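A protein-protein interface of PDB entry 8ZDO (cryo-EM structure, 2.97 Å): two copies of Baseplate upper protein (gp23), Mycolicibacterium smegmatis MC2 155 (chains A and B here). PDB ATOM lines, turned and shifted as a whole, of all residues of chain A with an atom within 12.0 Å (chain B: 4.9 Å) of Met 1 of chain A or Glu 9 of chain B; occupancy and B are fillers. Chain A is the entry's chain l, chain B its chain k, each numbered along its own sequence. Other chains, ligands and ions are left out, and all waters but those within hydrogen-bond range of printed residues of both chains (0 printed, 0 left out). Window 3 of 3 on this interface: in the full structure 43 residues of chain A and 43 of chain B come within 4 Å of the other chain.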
ATOM      1  N   MET A   1       2.224   9.783 -30.412  1.00  0.00           N
ATOM      2  CA  MET A   1       2.451  10.673 -29.282  1.00  0.00           C
ATOM      3  C   MET A   1       2.432   9.885 -27.981  1.00  0.00           C
ATOM      4  O   MET A   1       1.572  10.099 -27.131  1.00  0.00           O
ATOM      5  CB  MET A   1       1.397  11.777 -29.249  1.00  0.00           C
ATOM      6  CG  MET A   1       1.905  13.087 -28.691  1.00  0.00           C
ATOM      7  SD  MET A   1       3.427  13.597 -29.504  1.00  0.00           S
ATOM      8  CE  MET A   1       4.098  14.707 -28.276  1.00  0.00           C
ATOM      9  N   LEU A   2       3.388   8.967 -27.836  1.00  0.00           N
ATOM     10  CA  LEU A   2       3.397   8.081 -26.677  1.00  0.00           C
ATOM     11  C   LEU A   2       3.677   8.841 -25.386  1.00  0.00           C
ATOM     12  O   LEU A   2       3.063   8.561 -24.352  1.00  0.00           O
ATOM     13  CB  LEU A   2       4.429   6.974 -26.873  1.00  0.00           C
ATOM     14  CG  LEU A   2       4.137   5.931 -27.948  1.00  0.00           C
ATOM     15  CD1 LEU A   2       5.341   5.033 -28.137  1.00  0.00           C
ATOM     16  CD2 LEU A   2       2.910   5.119 -27.584  1.00  0.00           C
ATOM     17  N   SER A   3       4.601   9.793 -25.421  1.00  0.00           N
ATOM     18  CA  SER A   3       5.035  10.493 -24.221  1.00  0.00           C
ATOM     19  C   SER A   3       4.300  11.818 -24.078  1.00  0.00           C
ATOM     20  O   SER A   3       4.029  12.501 -25.069  1.00  0.00           O
ATOM     21  CB  SER A   3       6.543  10.736 -24.251  1.00  0.00           C
ATOM     22  OG  SER A   3       6.932  11.332 -25.472  1.00  0.00           O
ATOM     23  N   THR A   4       3.974  12.168 -22.837  1.00  0.00           N
ATOM     24  CA  THR A   4       3.340  13.449 -22.561  1.00  0.00           C
ATOM     25  C   THR A   4       4.308  14.592 -22.831  1.00  0.00           C
ATOM     26  O   THR A   4       5.496  14.511 -22.512  1.00  0.00           O
ATOM     27  CB  THR A   4       2.862  13.509 -21.113  1.00  0.00           C
ATOM     28  OG1 THR A   4       3.984  13.380 -20.233  1.00  0.00           O
ATOM     29  CG2 THR A   4       1.876  12.391 -20.836  1.00  0.00           C
ATOM     30  N   GLY A   5       3.790  15.666 -23.417  1.00  0.00           N
ATOM     31  CA  GLY A   5       4.598  16.815 -23.739  1.00  0.00           C
ATOM     32  C   GLY A   5       3.912  18.117 -23.391  1.00  0.00           C
ATOM     33  O   GLY A   5       2.716  18.159 -23.091  1.00  0.00           O
ATOM     34  N   PRO A   6       4.664  19.212 -23.422  1.00  0.00           N
ATOM     35  CA  PRO A   6       4.079  20.516 -23.115  1.00  0.00           C
ATOM     36  C   PRO A   6       3.178  21.001 -24.239  1.00  0.00           C
ATOM     37  O   PRO A   6       3.277  20.570 -25.389  1.00  0.00           O
ATOM     38  CB  PRO A   6       5.298  21.432 -22.951  1.00  0.00           C
ATOM     39  CG  PRO A   6       6.506  20.539 -23.037  1.00  0.00           C
ATOM     40  CD  PRO A   6       6.085  19.322 -23.778  1.00  0.00           C
ATOM     41  N   ILE A   7       2.286  21.918 -23.883  1.00  0.00           N
ATOM     42  CA  ILE A   7       1.420  22.593 -24.839  1.00  0.00           C
ATOM     43  C   ILE A   7       2.021  23.957 -25.137  1.00  0.00           C
ATOM     44  O   ILE A   7       2.313  24.727 -24.215  1.00  0.00           O
ATOM     45  CB  ILE A   7      -0.012  22.729 -24.299  1.00  0.00           C
ATOM     46  CG1 ILE A   7      -0.582  21.355 -23.943  1.00  0.00           C
ATOM     47  CG2 ILE A   7      -0.897  23.428 -25.312  1.00  0.00           C
ATOM     48  CD1 ILE A   7      -0.665  20.406 -25.115  1.00  0.00           C
ATOM     49  N   MET A   8       2.218  24.255 -26.418  1.00  0.00           N
ATOM     50  CA  MET A   8       2.737  25.560 -26.798  1.00  0.00           C
ATOM     51  C   MET A   8       1.692  26.630 -26.515  1.00  0.00           C
ATOM     52  O   MET A   8       0.558  26.552 -26.996  1.00  0.00           O
ATOM     53  CB  MET A   8       3.132  25.574 -28.273  1.00  0.00           C
ATOM     54  CG  MET A   8       4.066  26.715 -28.645  1.00  0.00           C
ATOM     55  SD  MET A   8       3.939  27.210 -30.375  1.00  0.00           S
ATOM     56  CE  MET A   8       4.744  25.836 -31.189  1.00  0.00           C
ATOM     57  N   GLN A  90       7.891  18.513 -14.201  1.00  0.00           N
ATOM     58  CA  GLN A  90       7.233  18.209 -15.464  1.00  0.00           C
ATOM     59  C   GLN A  90       6.743  19.510 -16.082  1.00  0.00           C
ATOM     60  O   GLN A  90       5.972  20.245 -15.457  1.00  0.00           O
ATOM     61  CB  GLN A  90       6.072  17.236 -15.256  1.00  0.00           C
ATOM     62  CG  GLN A  90       5.063  17.220 -16.382  1.00  0.00           C
ATOM     63  CD  GLN A  90       3.921  16.268 -16.112  1.00  0.00           C
ATOM     64  OE1 GLN A  90       3.878  15.612 -15.071  1.00  0.00           O
ATOM     65  NE2 GLN A  90       2.986  16.182 -17.050  1.00  0.00           N
ATOM     66  N   CYS A  91       7.184  19.788 -17.305  1.00  0.00           N
ATOM     67  CA  CYS A  91       6.839  21.035 -17.976  1.00  0.00           C
ATOM     68  C   CYS A  91       5.455  20.914 -18.600  1.00  0.00           C
ATOM     69  O   CYS A  91       5.220  20.042 -19.442  1.00  0.00           O
ATOM     70  CB  CYS A  91       7.883  21.370 -19.037  1.00  0.00           C
ATOM     71  SG  CYS A  91       7.405  22.686 -20.171  1.00  0.00           S
ATOM     72  N   LEU A  92       4.540  21.791 -18.189  1.00  0.00           N
ATOM     73  CA  LEU A  92       3.185  21.789 -18.725  1.00  0.00           C
ATOM     74  C   LEU A  92       3.056  22.670 -19.961  1.00  0.00           C
ATOM     75  O   LEU A  92       2.463  22.258 -20.961  1.00  0.00           O
ATOM     76  CB  LEU A  92       2.191  22.253 -17.659  1.00  0.00           C
ATOM     77  CG  LEU A  92       1.916  21.305 -16.496  1.00  0.00           C
ATOM     78  CD1 LEU A  92       0.775  21.847 -15.656  1.00  0.00           C
ATOM     79  CD2 LEU A  92       1.598  19.913 -17.007  1.00  0.00           C
ATOM     80  N   PHE A  94       5.030  25.843 -22.540  1.00  0.00           N
ATOM     81  CA  PHE A  94       6.199  26.593 -22.961  1.00  0.00           C
ATOM     82  C   PHE A  94       5.781  27.489 -24.113  1.00  0.00           C
ATOM     83  O   PHE A  94       4.778  27.236 -24.783  1.00  0.00           O
ATOM     84  CB  PHE A  94       7.352  25.672 -23.377  1.00  0.00           C
ATOM     85  CG  PHE A  94       7.198  25.088 -24.752  1.00  0.00           C
ATOM     86  CD1 PHE A  94       6.314  24.048 -24.981  1.00  0.00           C
ATOM     87  CD2 PHE A  94       7.934  25.576 -25.815  1.00  0.00           C
ATOM     88  CE1 PHE A  94       6.169  23.511 -26.240  1.00  0.00           C
ATOM     89  CE2 PHE A  94       7.791  25.041 -27.077  1.00  0.00           C
ATOM     90  CZ  PHE A  94       6.907  24.007 -27.289  1.00  0.00           C
ATOM     91  N   ILE B   7       4.236   0.243 -35.031  1.00  0.00           N
ATOM     92  CA  ILE B   7       3.465   1.452 -35.285  1.00  0.00           C
ATOM     93  C   ILE B   7       4.405   2.646 -35.226  1.00  0.00           C
ATOM     94  O   ILE B   7       5.223   2.758 -34.303  1.00  0.00           O
ATOM     95  CB  ILE B   7       2.319   1.606 -34.273  1.00  0.00           C
ATOM     96  CG1 ILE B   7       1.480   0.332 -34.222  1.00  0.00           C
ATOM     97  CG2 ILE B   7       1.451   2.796 -34.629  1.00  0.00           C
ATOM     98  CD1 ILE B   7       0.436   0.340 -33.134  1.00  0.00           C
ATOM     99  N   MET B   8       4.299   3.535 -36.210  1.00  0.00           N
ATOM    100  CA  MET B   8       5.130   4.732 -36.247  1.00  0.00           C
ATOM    101  C   MET B   8       4.492   5.807 -35.377  1.00  0.00           C
ATOM    102  O   MET B   8       3.394   6.289 -35.670  1.00  0.00           O
ATOM    103  CB  MET B   8       5.310   5.226 -37.678  1.00  0.00           C
ATOM    104  CG  MET B   8       6.409   6.262 -37.823  1.00  0.00           C
ATOM    105  SD  MET B   8       6.385   7.098 -39.418  1.00  0.00           S
ATOM    106  CE  MET B   8       6.873   5.767 -40.511  1.00  0.00           C
ATOM    107  N   GLU B   9       5.182   6.173 -34.301  1.00  0.00           N
ATOM    108  CA  GLU B   9       4.746   7.236 -33.408  1.00  0.00           C
ATOM    109  C   GLU B   9       5.896   8.210 -33.197  1.00  0.00           C
ATOM    110  O   GLU B   9       6.935   8.096 -33.852  1.00  0.00           O
ATOM    111  CB  GLU B   9       4.279   6.656 -32.071  1.00  0.00           C
ATOM    112  CG  GLU B   9       2.895   6.031 -32.105  1.00  0.00           C
ATOM    113  CD  GLU B   9       1.789   7.017 -31.785  1.00  0.00           C
ATOM    114  OE1 GLU B   9       1.943   8.215 -32.099  1.00  0.00           O
ATOM    115  OE2 GLU B   9       0.763   6.591 -31.215  1.00  0.00           O
ATOM    116  N   THR B  10       5.723   9.175 -32.298  1.00  0.00           N
ATOM    117  CA  THR B  10       6.817  10.035 -31.877  1.00  0.00           C
ATOM    118  C   THR B  10       6.806  10.176 -30.366  1.00  0.00           C
ATOM    119  O   THR B  10       5.746  10.143 -29.735  1.00  0.00           O
ATOM    120  CB  THR B  10       6.759  11.435 -32.515  1.00  0.00           C
ATOM    121  OG1 THR B  10       5.494  12.047 -32.235  1.00  0.00           O
ATOM    122  CG2 THR B  10       7.013  11.379 -34.014  1.00  0.00           C
ATOM    123  N   LEU B  11       7.996  10.308 -29.798  1.00  0.00           N
ATOM    124  CA  LEU B  11       8.187  10.709 -28.417  1.00  0.00           C
ATOM    125  C   LEU B  11       8.540  12.189 -28.384  1.00  0.00           C
ATOM    126  O   LEU B  11       8.959  12.768 -29.385  1.00  0.00           O
ATOM    127  CB  LEU B  11       9.291   9.883 -27.758  1.00  0.00           C
ATOM    128  CG  LEU B  11       8.991   8.394 -27.594  1.00  0.00           C
ATOM    129  CD1 LEU B  11      10.158   7.679 -26.956  1.00  0.00           C
ATOM    130  CD2 LEU B  11       7.745   8.204 -26.767  1.00  0.00           C
ATOM    131  N   THR B  12       8.353  12.804 -27.223  1.00  0.00           N
ATOM    132  CA  THR B  12       8.664  14.215 -27.050  1.00  0.00           C
ATOM    133  C   THR B  12       9.631  14.394 -25.890  1.00  0.00           C
ATOM    134  O   THR B  12       9.497  13.748 -24.847  1.00  0.00           O
ATOM    135  CB  THR B  12       7.394  15.043 -26.821  1.00  0.00           C
ATOM    136  OG1 THR B  12       7.747  16.414 -26.603  1.00  0.00           O
ATOM    137  CG2 THR B  12       6.614  14.524 -25.630  1.00  0.00           C
ATOM    138  N   LYS B  25      -1.337   4.633 -22.283  1.00  0.00           N
ATOM    139  CA  LYS B  25      -1.033   4.629 -23.706  1.00  0.00           C
ATOM    140  C   LYS B  25      -0.288   3.378 -24.146  1.00  0.00           C
ATOM    141  O   LYS B  25      -0.122   3.166 -25.351  1.00  0.00           O
ATOM    142  CB  LYS B  25      -0.213   5.869 -24.072  1.00  0.00           C
ATOM    143  CG  LYS B  25      -0.964   7.165 -23.859  1.00  0.00           C
ATOM    144  CD  LYS B  25      -0.043   8.361 -23.912  1.00  0.00           C
ATOM    145  CE  LYS B  25      -0.542   9.389 -24.907  1.00  0.00           C
ATOM    146  NZ  LYS B  25       0.391  10.542 -25.018  1.00  0.00           N
ATOM    147  N   PHE B  78      13.854   6.002 -32.359  1.00  0.00           N
ATOM    148  CA  PHE B  78      13.519   5.279 -31.143  1.00  0.00           C
ATOM    149  C   PHE B  78      12.721   4.037 -31.506  1.00  0.00           C
ATOM    150  O   PHE B  78      11.933   4.041 -32.456  1.00  0.00           O
ATOM    151  CB  PHE B  78      12.746   6.162 -30.149  1.00  0.00           C
ATOM    152  CG  PHE B  78      11.252   6.155 -30.344  1.00  0.00           C
ATOM    153  CD1 PHE B  78      10.457   5.208 -29.721  1.00  0.00           C
ATOM    154  CD2 PHE B  78      10.643   7.111 -31.133  1.00  0.00           C
ATOM    155  CE1 PHE B  78       9.094   5.206 -29.898  1.00  0.00           C
ATOM    156  CE2 PHE B  78       9.278   7.115 -31.307  1.00  0.00           C
ATOM    157  CZ  PHE B  78       8.503   6.161 -30.689  1.00  0.00           C
ATOM    158  N   TYR B  93       6.340  -0.076 -31.014  1.00  0.00           N
ATOM    159  CA  TYR B  93       6.354   1.265 -31.574  1.00  0.00           C
ATOM    160  C   TYR B  93       7.756   1.619 -32.037  1.00  0.00           C
ATOM    161  O   TYR B  93       8.750   1.088 -31.539  1.00  0.00           O
ATOM    162  CB  TYR B  93       5.882   2.307 -30.556  1.00  0.00           C
ATOM    163  CG  TYR B  93       4.440   2.156 -30.141  1.00  0.00           C
ATOM    164  CD1 TYR B  93       3.419   2.662 -30.923  1.00  0.00           C
ATOM    165  CD2 TYR B  93       4.103   1.508 -28.963  1.00  0.00           C
ATOM    166  CE1 TYR B  93       2.102   2.526 -30.550  1.00  0.00           C
ATOM    167  CE2 TYR B  93       2.788   1.366 -28.582  1.00  0.00           C
ATOM    168  CZ  TYR B  93       1.791   1.878 -29.379  1.00  0.00           C
ATOM    169  OH  TYR B  93       0.475   1.741 -29.002  1.00  0.00           O
ATOM    170  N   PHE B  94       7.822   2.527 -33.003  1.00  0.00           N
ATOM    171  CA  PHE B  94       9.090   3.076 -33.454  1.00  0.00           C
ATOM    172  C   PHE B  94       8.827   4.443 -34.060  1.00  0.00           C
ATOM    173  O   PHE B  94       7.693   4.784 -34.395  1.00  0.00           O
ATOM    174  CB  PHE B  94       9.785   2.156 -34.463  1.00  0.00           C
ATOM    175  CG  PHE B  94       9.344   2.368 -35.879  1.00  0.00           C
ATOM    176  CD1 PHE B  94       8.125   1.885 -36.318  1.00  0.00           C
ATOM    177  CD2 PHE B  94      10.148   3.050 -36.772  1.00  0.00           C
ATOM    178  CE1 PHE B  94       7.718   2.082 -37.618  1.00  0.00           C
ATOM    179  CE2 PHE B  94       9.744   3.247 -38.074  1.00  0.00           C
ATOM    180  CZ  PHE B  94       8.529   2.761 -38.496  1.00  0.00           C
ATOM    181  N   GLY B  95       9.882   5.224 -34.194  1.00  0.00           N
ATOM    182  CA  GLY B  95       9.708   6.537 -34.795  1.00  0.00           C
ATOM    183  C   GLY B  95      10.894   7.432 -34.496  1.00  0.00           C
ATOM    184  O   GLY B  95      12.012   6.955 -34.319  1.00  0.00           O
ATOM    185  N   THR B  96      10.623   8.733 -34.451  1.00  0.00           N
ATOM    186  CA  THR B  96      11.621   9.735 -34.111  1.00  0.00           C
ATOM    187  C   THR B  96      11.154  10.525 -32.898  1.00  0.00           C
ATOM    188  O   THR B  96       9.982  10.897 -32.802  1.00  0.00           O
ATOM    189  CB  THR B  96      11.879  10.696 -35.276  1.00  0.00           C
ATOM    190  OG1 THR B  96      10.741  11.546 -35.459  1.00  0.00           O
ATOM    191  CG2 THR B  96      12.144   9.930 -36.558  1.00  0.00           C
ATOM    192  N   LYS B 100      10.424  19.138 -28.060  1.00  0.00           N
ATOM    193  CA  LYS B 100       9.397  20.174 -27.946  1.00  0.00           C
ATOM    194  C   LYS B 100       9.765  21.063 -26.764  1.00  0.00           C
ATOM    195  O   LYS B 100       9.366  20.817 -25.627  1.00  0.00           O
ATOM    196  CB  LYS B 100       8.017  19.550 -27.782  1.00  0.00           C
ATOM    197  CG  LYS B 100       6.875  20.495 -28.088  1.00  0.00           C
ATOM    198  CD  LYS B 100       5.562  19.749 -28.212  1.00  0.00           C
ATOM    199  CE  LYS B 100       5.535  18.893 -29.463  1.00  0.00           C
ATOM    200  NZ  LYS B 100       4.252  18.155 -29.594  1.00  0.00           N
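OG1 of Thr 10 of chain B sits at hydrogen-bond distance from SD of Met 1 of chain A (3.8 Å).
O of Thr 10 of chain B is in hydrogen-bond range of N of Leu 2 of chain A, at 3.2 Å.
N of Thr 12 of chain B sits at hydrogen-bond distance from OG of Ser 3 of chain A (2.7 Å).
The side-chain amino group (NZ) of Lys 25 of chain B sits at hydrogen-bond distance from the backbone carbonyl oxygen (O) of Met 1 of chain A, at 2.5 Å.
O of Leu 2 of chain A sits close to NZ of Lys 25 of chain B (3.4 Å).
The side-chain carboxylate (OE1) of Glu 9 of chain B lies close to the backbone NH (N) of Met 1 of chain A.
3 positions are printed for both chains.
Of the 15 pairs that touch across the chains among the printed residues, none has its exchanged pair printed and touching as well.
CB of Thr 12 of chain B touches CE of Met 1 of chain A, at 3.6 Å.
Met 1 of chain A touches Lys 100 of chain B.
CB of Leu 2 of chain A touches CD2 of Leu 11 of chain B, at 3.5 Å.
Tyr 93 of chain B touches Leu 2 of chain A (CG to CD1, 3.6 Å).
CA of Leu 11 of chain B touches OG of Ser 3 of chain A (3.3 Å).
Thr 4 of chain A touches Thr 12 of chain B (O to CG2, 3.3 Å).
Gly 5 of chain A touches Thr 12 of chain B (CA to CG2, 3.6 Å).
O of Pro 6 of chain A touches CD of Lys 100 of chain B, at 3.7 Å.
CG of Lys 100 of chain B touches CZ of Phe 94 of chain A (3.6 Å).
Of chain B, only Glu 9, Thr 10, Thr 12, Lys 25 and Lys 100 come within 4 Å of Met 1 of chain A.
Of the printed residues of chain B, Pro 6 of chain A touches Lys 100 (3.7 Å).
Ile 7 of chain A touches none of the printed residues of chain B.
Cys 91 of chain A touches none of the printed residues of chain B.
Ile 7 of chain B touches none of the printed residues of chain A.
No residue of chain A comes within 4 Å of Met 8 of chain B.
Of the printed residues of chain A, Glu 9 of chain B touches Met 1.
Leu 11 of chain B touches just these residues of chain A: Leu 2 and Ser 3.
Thr 12 of chain B touches four residues of chain A.
Lys 25 of chain B touches just these residues of chain A: Met 1 (2.5 Å) and Leu 2 (3.1 Å).
No residue of chain A comes within 4 Å of Phe 78 of chain B.
Tyr 93 of chain B touches one residue of chain A.
No residue of chain A comes within 4 Å of Gly 95 of chain B.
Printed residues of chain A within 4 Å of Lys 100 of chain B: Met 1 (3.7 Å), Pro 6 (3.7 Å) and Phe 94 (3.6 Å).
The backbone carbonyl oxygen (O) of Phe 94 of chain B sits at hydrogen-bond distance from the backbone NH (N) of Glu 9 of chain B (2.9 Å).
The backbone carbonyl oxygen (O) of Ile 7 of chain A is in hydrogen-bond range of the backbone NH (N) of Phe 94 of chain A (3.4 Å).
Hydrophobic or aromatic side chains of chain A within 4 Å of the printed part of chain B: Met 1, Leu 2, Pro 6 and Phe 94.
Along chain A the printed residues that touch a printed residue of chain B span positions 1 to 94.
Of the 13 printed residues of chain B, 7 touch a printed residue of chain A.
Among the printed residues, 15 pairs touch across the chains.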
